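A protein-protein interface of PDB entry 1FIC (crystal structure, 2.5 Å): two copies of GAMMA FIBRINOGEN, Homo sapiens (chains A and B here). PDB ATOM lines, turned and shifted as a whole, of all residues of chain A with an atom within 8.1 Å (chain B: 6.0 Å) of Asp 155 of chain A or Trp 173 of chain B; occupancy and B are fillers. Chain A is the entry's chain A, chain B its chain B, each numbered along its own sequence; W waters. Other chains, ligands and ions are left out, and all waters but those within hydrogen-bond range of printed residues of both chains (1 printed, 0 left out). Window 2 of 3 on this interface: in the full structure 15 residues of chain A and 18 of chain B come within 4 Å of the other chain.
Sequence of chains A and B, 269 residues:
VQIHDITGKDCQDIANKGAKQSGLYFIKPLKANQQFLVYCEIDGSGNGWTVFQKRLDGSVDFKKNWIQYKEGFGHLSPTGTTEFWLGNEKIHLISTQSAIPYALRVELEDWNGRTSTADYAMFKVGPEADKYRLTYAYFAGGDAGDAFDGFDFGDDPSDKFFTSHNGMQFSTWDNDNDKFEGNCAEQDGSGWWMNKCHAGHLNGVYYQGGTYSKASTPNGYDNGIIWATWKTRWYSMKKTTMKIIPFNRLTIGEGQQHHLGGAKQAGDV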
ATOM      1  N   PHE A 151      17.507 -11.994  23.661  1.00  0.00           N
ATOM      2  CA  PHE A 151      17.660 -13.392  23.994  1.00  0.00           C
ATOM      3  C   PHE A 151      18.223 -14.159  22.800  1.00  0.00           C
ATOM      4  O   PHE A 151      17.885 -13.860  21.665  1.00  0.00           O
ATOM      5  CB  PHE A 151      16.311 -13.962  24.433  1.00  0.00           C
ATOM      6  CG  PHE A 151      16.404 -15.322  25.037  1.00  0.00           C
ATOM      7  CD1 PHE A 151      16.877 -15.487  26.324  1.00  0.00           C
ATOM      8  CD2 PHE A 151      16.054 -16.445  24.305  1.00  0.00           C
ATOM      9  CE1 PHE A 151      17.004 -16.753  26.877  1.00  0.00           C
ATOM     10  CE2 PHE A 151      16.181 -17.714  24.843  1.00  0.00           C
ATOM     11  CZ  PHE A 151      16.660 -17.867  26.136  1.00  0.00           C
ATOM     12  N   ASP A 152      19.134 -15.096  23.046  1.00  0.00           N
ATOM     13  CA  ASP A 152      19.703 -15.882  21.954  1.00  0.00           C
ATOM     14  C   ASP A 152      18.902 -17.160  21.741  1.00  0.00           C
ATOM     15  O   ASP A 152      19.266 -18.205  22.251  1.00  0.00           O
ATOM     16  CB  ASP A 152      21.168 -16.246  22.230  1.00  0.00           C
ATOM     17  CG  ASP A 152      22.018 -16.263  20.954  1.00  0.00           C
ATOM     18  OD1 ASP A 152      21.621 -16.919  19.947  1.00  0.00           O
ATOM     19  OD2 ASP A 152      23.075 -15.584  20.957  1.00  0.00           O
ATOM     20  N   PHE A 153      17.804 -17.070  21.002  1.00  0.00           N
ATOM     21  CA  PHE A 153      16.976 -18.233  20.733  1.00  0.00           C
ATOM     22  C   PHE A 153      17.791 -19.305  20.023  1.00  0.00           C
ATOM     23  O   PHE A 153      17.482 -20.491  20.114  1.00  0.00           O
ATOM     24  CB  PHE A 153      15.772 -17.841  19.876  1.00  0.00           C
ATOM     25  CG  PHE A 153      14.853 -16.884  20.545  1.00  0.00           C
ATOM     26  CD1 PHE A 153      14.031 -17.311  21.579  1.00  0.00           C
ATOM     27  CD2 PHE A 153      14.833 -15.544  20.167  1.00  0.00           C
ATOM     28  CE1 PHE A 153      13.197 -16.414  22.238  1.00  0.00           C
ATOM     29  CE2 PHE A 153      14.008 -14.636  20.809  1.00  0.00           C
ATOM     30  CZ  PHE A 153      13.183 -15.063  21.852  1.00  0.00           C
ATOM     31  N   GLY A 154      18.828 -18.876  19.313  1.00  0.00           N
ATOM     32  CA  GLY A 154      19.674 -19.810  18.602  1.00  0.00           C
ATOM     33  C   GLY A 154      19.334 -19.953  17.130  1.00  0.00           C
ATOM     34  O   GLY A 154      20.127 -20.510  16.368  1.00  0.00           O
ATOM     35  N   ASP A 155      18.182 -19.423  16.724  1.00  0.00           N
ATOM     36  CA  ASP A 155      17.726 -19.486  15.335  1.00  0.00           C
ATOM     37  C   ASP A 155      18.624 -18.716  14.397  1.00  0.00           C
ATOM     38  O   ASP A 155      18.733 -19.050  13.213  1.00  0.00           O
ATOM     39  CB  ASP A 155      16.302 -18.951  15.209  1.00  0.00           C
ATOM     40  CG  ASP A 155      15.322 -19.701  16.081  1.00  0.00           C
ATOM     41  OD1 ASP A 155      15.464 -20.933  16.246  1.00  0.00           O
ATOM     42  OD2 ASP A 155      14.407 -19.045  16.609  1.00  0.00           O
ATOM     43  N   ASP A 156      19.202 -17.642  14.916  1.00  0.00           N
ATOM     44  CA  ASP A 156      20.121 -16.805  14.161  1.00  0.00           C
ATOM     45  C   ASP A 156      21.161 -16.342  15.173  1.00  0.00           C
ATOM     46  O   ASP A 156      20.858 -16.186  16.362  1.00  0.00           O
ATOM     47  CB  ASP A 156      19.392 -15.598  13.547  1.00  0.00           C
ATOM     48  CG  ASP A 156      20.209 -14.891  12.462  1.00  0.00           C
ATOM     49  OD1 ASP A 156      21.013 -13.989  12.794  1.00  0.00           O
ATOM     50  OD2 ASP A 156      20.044 -15.244  11.273  1.00  0.00           O
ATOM     51  N   PRO A 157      22.412 -16.165  14.728  1.00  0.00           N
ATOM     52  CA  PRO A 157      23.500 -15.724  15.606  1.00  0.00           C
ATOM     53  C   PRO A 157      23.253 -14.339  16.204  1.00  0.00           C
ATOM     54  O   PRO A 157      23.668 -14.043  17.334  1.00  0.00           O
ATOM     55  CB  PRO A 157      24.702 -15.716  14.662  1.00  0.00           C
ATOM     56  CG  PRO A 157      24.371 -16.821  13.698  1.00  0.00           C
ATOM     57  CD  PRO A 157      22.933 -16.531  13.397  1.00  0.00           C
ATOM     58  N   SER A 158      22.540 -13.504  15.458  1.00  0.00           N
ATOM     59  CA  SER A 158      22.257 -12.153  15.918  1.00  0.00           C
ATOM     60  C   SER A 158      20.949 -11.976  16.719  1.00  0.00           C
ATOM     61  O   SER A 158      20.606 -10.862  17.096  1.00  0.00           O
ATOM     62  CB  SER A 158      22.312 -11.201  14.722  1.00  0.00           C
ATOM     63  OG  SER A 158      23.479 -11.438  13.938  1.00  0.00           O
ATOM     64  N   ASP A 159      20.243 -13.068  17.010  1.00  0.00           N
ATOM     65  CA  ASP A 159      18.993 -13.028  17.772  1.00  0.00           C
ATOM     66  C   ASP A 159      19.041 -12.049  18.912  1.00  0.00           C
ATOM     67  O   ASP A 159      18.154 -11.238  19.079  1.00  0.00           O
ATOM     68  CB  ASP A 159      18.717 -14.376  18.410  1.00  0.00           C
ATOM     69  CG  ASP A 159      18.184 -15.371  17.450  1.00  0.00           C
ATOM     70  OD1 ASP A 159      17.636 -14.979  16.396  1.00  0.00           O
ATOM     71  OD2 ASP A 159      18.300 -16.557  17.771  1.00  0.00           O
ATOM     72  N   LYS A 160      20.066 -12.195  19.738  1.00  0.00           N
ATOM     73  CA  LYS A 160      20.267 -11.362  20.906  1.00  0.00           C
ATOM     74  C   LYS A 160      20.235  -9.897  20.505  1.00  0.00           C
ATOM     75  O   LYS A 160      19.544  -9.091  21.111  1.00  0.00           O
ATOM     76  CB  LYS A 160      21.596 -11.746  21.554  1.00  0.00           C
ATOM     77  CG  LYS A 160      22.022 -10.881  22.706  1.00  0.00           C
ATOM     78  CD  LYS A 160      21.482 -11.371  24.022  1.00  0.00           C
ATOM     79  CE  LYS A 160      21.926 -10.455  25.158  1.00  0.00           C
ATOM     80  NZ  LYS A 160      21.581 -11.044  26.479  1.00  0.00           N
ATOM     81  N   LYS A 214       3.192 -22.622  16.855  1.00  0.00           N
ATOM     82  CA  LYS A 214       3.358 -22.105  15.508  1.00  0.00           C
ATOM     83  C   LYS A 214       2.080 -22.258  14.698  1.00  0.00           C
ATOM     84  O   LYS A 214       1.879 -21.572  13.703  1.00  0.00           O
ATOM     85  CB  LYS A 214       4.517 -22.849  14.848  1.00  0.00           C
ATOM     86  CG  LYS A 214       4.848 -22.427  13.437  1.00  0.00           C
ATOM     87  CD  LYS A 214       6.116 -23.131  12.950  1.00  0.00           C
ATOM     88  CE  LYS A 214       7.348 -22.687  13.743  1.00  0.00           C
ATOM     89  NZ  LYS A 214       7.651 -21.222  13.571  1.00  0.00           N
ATOM     90  N   ASP A 222       5.303 -16.156  17.160  1.00  0.00           N
ATOM     91  CA  ASP A 222       5.416 -16.335  18.610  1.00  0.00           C
ATOM     92  C   ASP A 222       4.897 -15.005  19.179  1.00  0.00           C
ATOM     93  O   ASP A 222       5.640 -14.170  19.697  1.00  0.00           O
ATOM     94  CB  ASP A 222       6.850 -16.656  19.071  1.00  0.00           C
ATOM     95  CG  ASP A 222       7.889 -15.691  18.553  1.00  0.00           C
ATOM     96  OD1 ASP A 222       7.683 -14.994  17.538  1.00  0.00           O
ATOM     97  OD2 ASP A 222       8.957 -15.654  19.168  1.00  0.00           O
ATOM     98  N   ARG A 233       9.461 -19.337  24.344  1.00  0.00           N
ATOM     99  CA  ARG A 233       8.768 -18.385  23.471  1.00  0.00           C
ATOM    100  C   ARG A 233       7.338 -18.794  23.112  1.00  0.00           C
ATOM    101  O   ARG A 233       6.603 -18.004  22.493  1.00  0.00           O
ATOM    102  CB  ARG A 233       9.546 -18.174  22.189  1.00  0.00           C
ATOM    103  CG  ARG A 233       9.482 -19.366  21.284  1.00  0.00           C
ATOM    104  CD  ARG A 233      10.618 -19.380  20.328  1.00  0.00           C
ATOM    105  NE  ARG A 233      10.618 -18.209  19.475  1.00  0.00           N
ATOM    106  CZ  ARG A 233      11.642 -17.864  18.700  1.00  0.00           C
ATOM    107  NH1 ARG A 233      12.743 -18.605  18.679  1.00  0.00           N
ATOM    108  NH2 ARG A 233      11.560 -16.789  17.934  1.00  0.00           N
ATOM    109  N   TRP A 234       6.975 -20.039  23.444  1.00  0.00           N
ATOM    110  CA  TRP A 234       5.639 -20.573  23.171  1.00  0.00           C
ATOM    111  C   TRP A 234       4.883 -20.729  24.479  1.00  0.00           C
ATOM    112  O   TRP A 234       4.126 -21.704  24.664  1.00  0.00           O
ATOM    113  CB  TRP A 234       5.685 -21.923  22.433  1.00  0.00           C
ATOM    114  CG  TRP A 234       6.425 -21.868  21.161  1.00  0.00           C
ATOM    115  CD1 TRP A 234       7.668 -22.376  20.922  1.00  0.00           C
ATOM    116  CD2 TRP A 234       6.048 -21.149  19.974  1.00  0.00           C
ATOM    117  NE1 TRP A 234       8.107 -21.994  19.670  1.00  0.00           N
ATOM    118  CE2 TRP A 234       7.132 -21.237  19.070  1.00  0.00           C
ATOM    119  CE3 TRP A 234       4.906 -20.428  19.594  1.00  0.00           C
ATOM    120  CZ2 TRP A 234       7.112 -20.625  17.810  1.00  0.00           C
ATOM    121  CZ3 TRP A 234       4.885 -19.825  18.342  1.00  0.00           C
ATOM    122  CH2 TRP A 234       5.983 -19.926  17.468  1.00  0.00           C
ATOM    123  N   LYS B  63      15.259 -26.065  22.482  1.00  0.00           N
ATOM    124  CA  LYS B  63      15.507 -26.037  21.058  1.00  0.00           C
ATOM    125  C   LYS B  63      16.633 -25.028  20.857  1.00  0.00           C
ATOM    126  O   LYS B  63      16.413 -23.846  20.596  1.00  0.00           O
ATOM    127  CB  LYS B  63      14.277 -25.656  20.231  1.00  0.00           C
ATOM    128  CG  LYS B  63      14.620 -25.568  18.749  1.00  0.00           C
ATOM    129  CD  LYS B  63      13.412 -25.467  17.859  1.00  0.00           C
ATOM    130  CE  LYS B  63      13.837 -25.378  16.381  1.00  0.00           C
ATOM    131  NZ  LYS B  63      12.692 -25.567  15.399  1.00  0.00           N
ATOM    132  N   LYS B  64      17.841 -25.503  21.076  1.00  0.00           N
ATOM    133  CA  LYS B  64      19.021 -24.690  20.923  1.00  0.00           C
ATOM    134  C   LYS B  64      19.765 -25.247  19.723  1.00  0.00           C
ATOM    135  O   LYS B  64      19.471 -26.358  19.269  1.00  0.00           O
ATOM    136  CB  LYS B  64      19.874 -24.814  22.179  1.00  0.00           C
ATOM    137  CG  LYS B  64      19.184 -24.337  23.429  1.00  0.00           C
ATOM    138  CD  LYS B  64      19.049 -22.835  23.433  1.00  0.00           C
ATOM    139  CE  LYS B  64      18.371 -22.388  24.708  1.00  0.00           C
ATOM    140  NZ  LYS B  64      17.139 -21.606  24.443  1.00  0.00           N
ATOM    141  N   ASN B  65      20.693 -24.467  19.179  1.00  0.00           N
ATOM    142  CA  ASN B  65      21.467 -24.901  18.034  1.00  0.00           C
ATOM    143  C   ASN B  65      22.674 -25.700  18.507  1.00  0.00           C
ATOM    144  O   ASN B  65      22.853 -25.910  19.705  1.00  0.00           O
ATOM    145  CB  ASN B  65      21.884 -23.707  17.149  1.00  0.00           C
ATOM    146  CG  ASN B  65      22.774 -22.674  17.877  1.00  0.00           C
ATOM    147  OD1 ASN B  65      23.534 -23.011  18.788  1.00  0.00           O
ATOM    148  ND2 ASN B  65      22.702 -21.415  17.435  1.00  0.00           N
ATOM    149  N   TRP B  66      23.515 -26.110  17.564  1.00  0.00           N
ATOM    150  CA  TRP B  66      24.706 -26.895  17.858  1.00  0.00           C
ATOM    151  C   TRP B  66      25.666 -26.261  18.852  1.00  0.00           C
ATOM    152  O   TRP B  66      26.098 -26.930  19.786  1.00  0.00           O
ATOM    153  CB  TRP B  66      25.458 -27.225  16.573  1.00  0.00           C
ATOM    154  CG  TRP B  66      26.642 -28.133  16.787  1.00  0.00           C
ATOM    155  CD1 TRP B  66      27.949 -27.753  16.894  1.00  0.00           C
ATOM    156  CD2 TRP B  66      26.627 -29.571  16.900  1.00  0.00           C
ATOM    157  NE1 TRP B  66      28.741 -28.855  17.063  1.00  0.00           N
ATOM    158  CE2 TRP B  66      27.962 -29.984  17.070  1.00  0.00           C
ATOM    159  CE3 TRP B  66      25.616 -30.547  16.878  1.00  0.00           C
ATOM    160  CZ2 TRP B  66      28.317 -31.338  17.217  1.00  0.00           C
ATOM    161  CZ3 TRP B  66      25.971 -31.901  17.027  1.00  0.00           C
ATOM    162  CH2 TRP B  66      27.308 -32.275  17.193  1.00  0.00           C
ATOM    163  N   GLN B  68      25.133 -23.931  21.080  1.00  0.00           N
ATOM    164  CA  GLN B  68      24.509 -23.810  22.383  1.00  0.00           C
ATOM    165  C   GLN B  68      24.551 -25.148  23.099  1.00  0.00           C
ATOM    166  O   GLN B  68      24.925 -25.223  24.262  1.00  0.00           O
ATOM    167  CB  GLN B  68      23.068 -23.306  22.242  1.00  0.00           C
ATOM    168  CG  GLN B  68      22.971 -21.891  21.666  1.00  0.00           C
ATOM    169  CD  GLN B  68      21.548 -21.455  21.360  1.00  0.00           C
ATOM    170  OE1 GLN B  68      20.830 -22.137  20.651  1.00  0.00           O
ATOM    171  NE2 GLN B  68      21.142 -20.313  21.894  1.00  0.00           N
ATOM    172  N   SER B 171      22.608 -34.559  17.462  1.00  0.00           N
ATOM    173  CA  SER B 171      22.010 -33.792  16.385  1.00  0.00           C
ATOM    174  C   SER B 171      21.224 -32.624  16.973  1.00  0.00           C
ATOM    175  O   SER B 171      20.662 -32.736  18.074  1.00  0.00           O
ATOM    176  CB  SER B 171      21.082 -34.671  15.554  1.00  0.00           C
ATOM    177  OG  SER B 171      21.783 -35.770  15.004  1.00  0.00           O
ATOM    178  N   THR B 172      21.242 -31.498  16.261  1.00  0.00           N
ATOM    179  CA  THR B 172      20.508 -30.283  16.631  1.00  0.00           C
ATOM    180  C   THR B 172      19.848 -29.879  15.312  1.00  0.00           C
ATOM    181  O   THR B 172      20.290 -30.324  14.254  1.00  0.00           O
ATOM    182  CB  THR B 172      21.447 -29.159  17.085  1.00  0.00           C
ATOM    183  OG1 THR B 172      22.447 -28.948  16.089  1.00  0.00           O
ATOM    184  CG2 THR B 172      22.103 -29.484  18.422  1.00  0.00           C
ATOM    185  N   TRP B 173      18.811 -29.053  15.341  1.00  0.00           N
ATOM    186  CA  TRP B 173      18.163 -28.676  14.084  1.00  0.00           C
ATOM    187  C   TRP B 173      19.139 -28.205  13.006  1.00  0.00           C
ATOM    188  O   TRP B 173      18.904 -28.438  11.818  1.00  0.00           O
ATOM    189  CB  TRP B 173      17.068 -27.612  14.306  1.00  0.00           C
ATOM    190  CG  TRP B 173      17.571 -26.235  14.711  1.00  0.00           C
ATOM    191  CD1 TRP B 173      17.740 -25.763  15.983  1.00  0.00           C
ATOM    192  CD2 TRP B 173      18.022 -25.185  13.833  1.00  0.00           C
ATOM    193  NE1 TRP B 173      18.276 -24.496  15.948  1.00  0.00           N
ATOM    194  CE2 TRP B 173      18.461 -24.124  14.644  1.00  0.00           C
ATOM    195  CE3 TRP B 173      18.105 -25.050  12.435  1.00  0.00           C
ATOM    196  CZ2 TRP B 173      18.977 -22.950  14.114  1.00  0.00           C
ATOM    197  CZ3 TRP B 173      18.625 -23.875  11.906  1.00  0.00           C
ATOM    198  CH2 TRP B 173      19.053 -22.844  12.744  1.00  0.00           C
ATOM    199  N   ASP B 174      20.243 -27.579  13.417  1.00  0.00           N
ATOM    200  CA  ASP B 174      21.231 -27.057  12.466  1.00  0.00           C
ATOM    201  C   ASP B 174      22.444 -27.944  12.203  1.00  0.00           C
ATOM    202  O   ASP B 174      23.414 -27.514  11.561  1.00  0.00           O
ATOM    203  CB  ASP B 174      21.730 -25.676  12.919  1.00  0.00           C
ATOM    204  CG  ASP B 174      22.415 -25.715  14.270  1.00  0.00           C
ATOM    205  OD1 ASP B 174      21.963 -26.496  15.122  1.00  0.00           O
ATOM    206  OD2 ASP B 174      23.394 -24.967  14.484  1.00  0.00           O
ATOM    207  N   ASN B 175      22.424 -29.160  12.728  1.00  0.00           N
ATOM    208  CA  ASN B 175      23.544 -30.077  12.545  1.00  0.00           C
ATOM    209  C   ASN B 175      22.942 -31.454  12.685  1.00  0.00           C
ATOM    210  O   ASN B 175      22.932 -32.040  13.770  1.00  0.00           O
ATOM    211  CB  ASN B 175      24.600 -29.843  13.621  1.00  0.00           C
ATOM    212  CG  ASN B 175      25.936 -30.430  13.257  1.00  0.00           C
ATOM    213  OD1 ASN B 175      26.022 -31.415  12.522  1.00  0.00           O
ATOM    214  ND2 ASN B 175      26.997 -29.810  13.740  1.00  0.00           N
ATOM    215  N   ASP B 176      22.335 -31.908  11.598  1.00  0.00           N
ATOM    216  CA  ASP B 176      21.671 -33.197  11.554  1.00  0.00           C
ATOM    217  C   ASP B 176      22.646 -34.352  11.369  1.00  0.00           C
ATOM    218  O   ASP B 176      23.442 -34.358  10.423  1.00  0.00           O
ATOM    219  CB  ASP B 176      20.644 -33.166  10.426  1.00  0.00           C
ATOM    220  CG  ASP B 176      19.917 -34.467  10.248  1.00  0.00           C
ATOM    221  OD1 ASP B 176      19.782 -35.251  11.209  1.00  0.00           O
ATOM    222  OD2 ASP B 176      19.465 -34.693   9.118  1.00  0.00           O
ATOM    223  N   ASN B 183      14.891 -34.769   9.556  1.00  0.00           N
ATOM    224  CA  ASN B 183      15.603 -34.179  10.697  1.00  0.00           C
ATOM    225  C   ASN B 183      14.849 -34.333  12.021  1.00  0.00           C
ATOM    226  O   ASN B 183      13.972 -33.542  12.341  1.00  0.00           O
ATOM    227  CB  ASN B 183      15.885 -32.699  10.416  1.00  0.00           C
ATOM    228  CG  ASN B 183      16.818 -32.076  11.422  1.00  0.00           C
ATOM    229  OD1 ASN B 183      16.912 -32.525  12.559  1.00  0.00           O
ATOM    230  ND2 ASN B 183      17.511 -31.024  11.011  1.00  0.00           N
ATOM    231  N   ALA B 185      15.930 -33.752  15.023  1.00  0.00           N
ATOM    232  CA  ALA B 185      16.196 -32.632  15.926  1.00  0.00           C
ATOM    233  C   ALA B 185      15.297 -31.447  15.640  1.00  0.00           C
ATOM    234  O   ALA B 185      14.753 -30.830  16.553  1.00  0.00           O
ATOM    235  CB  ALA B 185      17.637 -32.218  15.830  1.00  0.00           C
ATOM    236  N   GLU B 186      15.138 -31.134  14.362  1.00  0.00           N
ATOM    237  CA  GLU B 186      14.301 -30.023  13.934  1.00  0.00           C
ATOM    238  C   GLU B 186      12.818 -30.275  14.145  1.00  0.00           C
ATOM    239  O   GLU B 186      12.111 -29.430  14.693  1.00  0.00           O
ATOM    240  CB  GLU B 186      14.557 -29.716  12.475  1.00  0.00           C
ATOM    241  CG  GLU B 186      13.658 -28.681  11.901  1.00  0.00           C
ATOM    242  CD  GLU B 186      14.013 -28.390  10.463  1.00  0.00           C
ATOM    243  OE1 GLU B 186      13.638 -29.197   9.562  1.00  0.00           O
ATOM    244  OE2 GLU B 186      14.695 -27.360  10.242  1.00  0.00           O
ATOM    245  N   SER B 190      14.719 -30.119  19.337  1.00  0.00           N
ATOM    246  CA  SER B 190      15.623 -30.404  20.442  1.00  0.00           C
ATOM    247  C   SER B 190      17.008 -30.816  20.002  1.00  0.00           C
ATOM    248  O   SER B 190      17.340 -30.764  18.825  1.00  0.00           O
ATOM    249  CB  SER B 190      15.049 -31.506  21.331  1.00  0.00           C
ATOM    250  OG  SER B 190      15.088 -32.739  20.655  1.00  0.00           O
ATOM    251  N   GLY B 191      17.836 -31.160  20.976  1.00  0.00           N
ATOM    252  CA  GLY B 191      19.176 -31.615  20.683  1.00  0.00           C
ATOM    253  C   GLY B 191      19.251 -32.939  21.400  1.00  0.00           C
ATOM    254  O   GLY B 191      18.953 -32.999  22.594  1.00  0.00           O
HETATM  255  O   HOH W   1      23.637 -18.847  18.505  1.00  0.00           O
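Water W1 bridges ND2 of Asn 65 of chain B (2.9 Å) and OD1 of Asp 152 of chain A (3.1 Å).
Of the 16 printed residues of chain B, 4 touch a printed residue of chain A.
Among the printed residues, 7 pairs touch across the chains.
Of chain B, only Trp 173 (3.8 Å) comes within 4 Å of Asp 155 of chain A.
Trp 173 of chain B touches just these residues of chain A: Gly 154 (3.5 Å) and Asp 155 (3.8 Å).
Of the printed residues of chain A, Gln 68 of chain B touches Asp 152, Phe 153 and Gly 154.
Printed residues of chain B within 4 Å of Gly 154 of chain A: Asn 65 (2.9 Å), Gln 68 (3.3 Å) and Trp 173 (3.5 Å).
Of the printed residues of chain A, Asn 65 of chain B touches Gly 154 (2.9 Å).
Of the printed residues of chain A, Lys 63 of chain B touches Phe 153 (3.6 Å).
Printed residues of chain B within 4 Å of Phe 153 of chain A: Lys 63 and Gln 68.
The nearest residue of chain A that does not touch Trp 173 of chain B is Asp 156 of chain A (5.4 Å).
Among the printed residues, pairs that only touch across the chains: Phe 153 of chain A with Lys 63 of chain B (3.6 Å), Phe 153 of chain A with Gln 68 of chain B (3.8 Å), Gly 154 of chain A with Gln 68 of chain B (3.3 Å), Gly 154 of chain A with Trp 173 of chain B (3.5 Å) and Asp 155 of chain A with Trp 173 of chain B (3.8 Å).
ND2 of Asn 65 of chain B lies within hydrogen-bond range of O of Gly 154 of chain A (2.9 Å).
O of Asp 152 of chain A sits at hydrogen-bond distance from NE2 of Gln 68 of chain B.
No position is printed for both chains.
The side-chain carboxylate (OD2) of Asp 159 of chain A sits at hydrogen-bond distance from the backbone NH (N) of Asp 155 of chain A (3.1 Å).
The side-chain carboxylate (OD1) of Asp 152 of chain A sits close to the backbone NH (N) of Gly 154 of chain A.
The side-chain amide nitrogen of Asn 183 of chain B lies within hydrogen-bond range of the backbone carbonyl oxygen of Trp 173 of chain B, 3.0 Å away.
N of Phe 153 of chain A sits at hydrogen-bond distance from OD2 of Asp 159 of chain A, at 3.3 Å.
The side-chain carboxylate (OD2) of Asp 155 of chain A is in salt-bridge range of the guanidinium group (NH1) of Arg 233 of chain A, at 2.7 Å.
The side-chain amide oxygen of Gln 68 of chain B is in hydrogen-bond range of the backbone NH of Asn 65 of chain B (2.8 Å).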
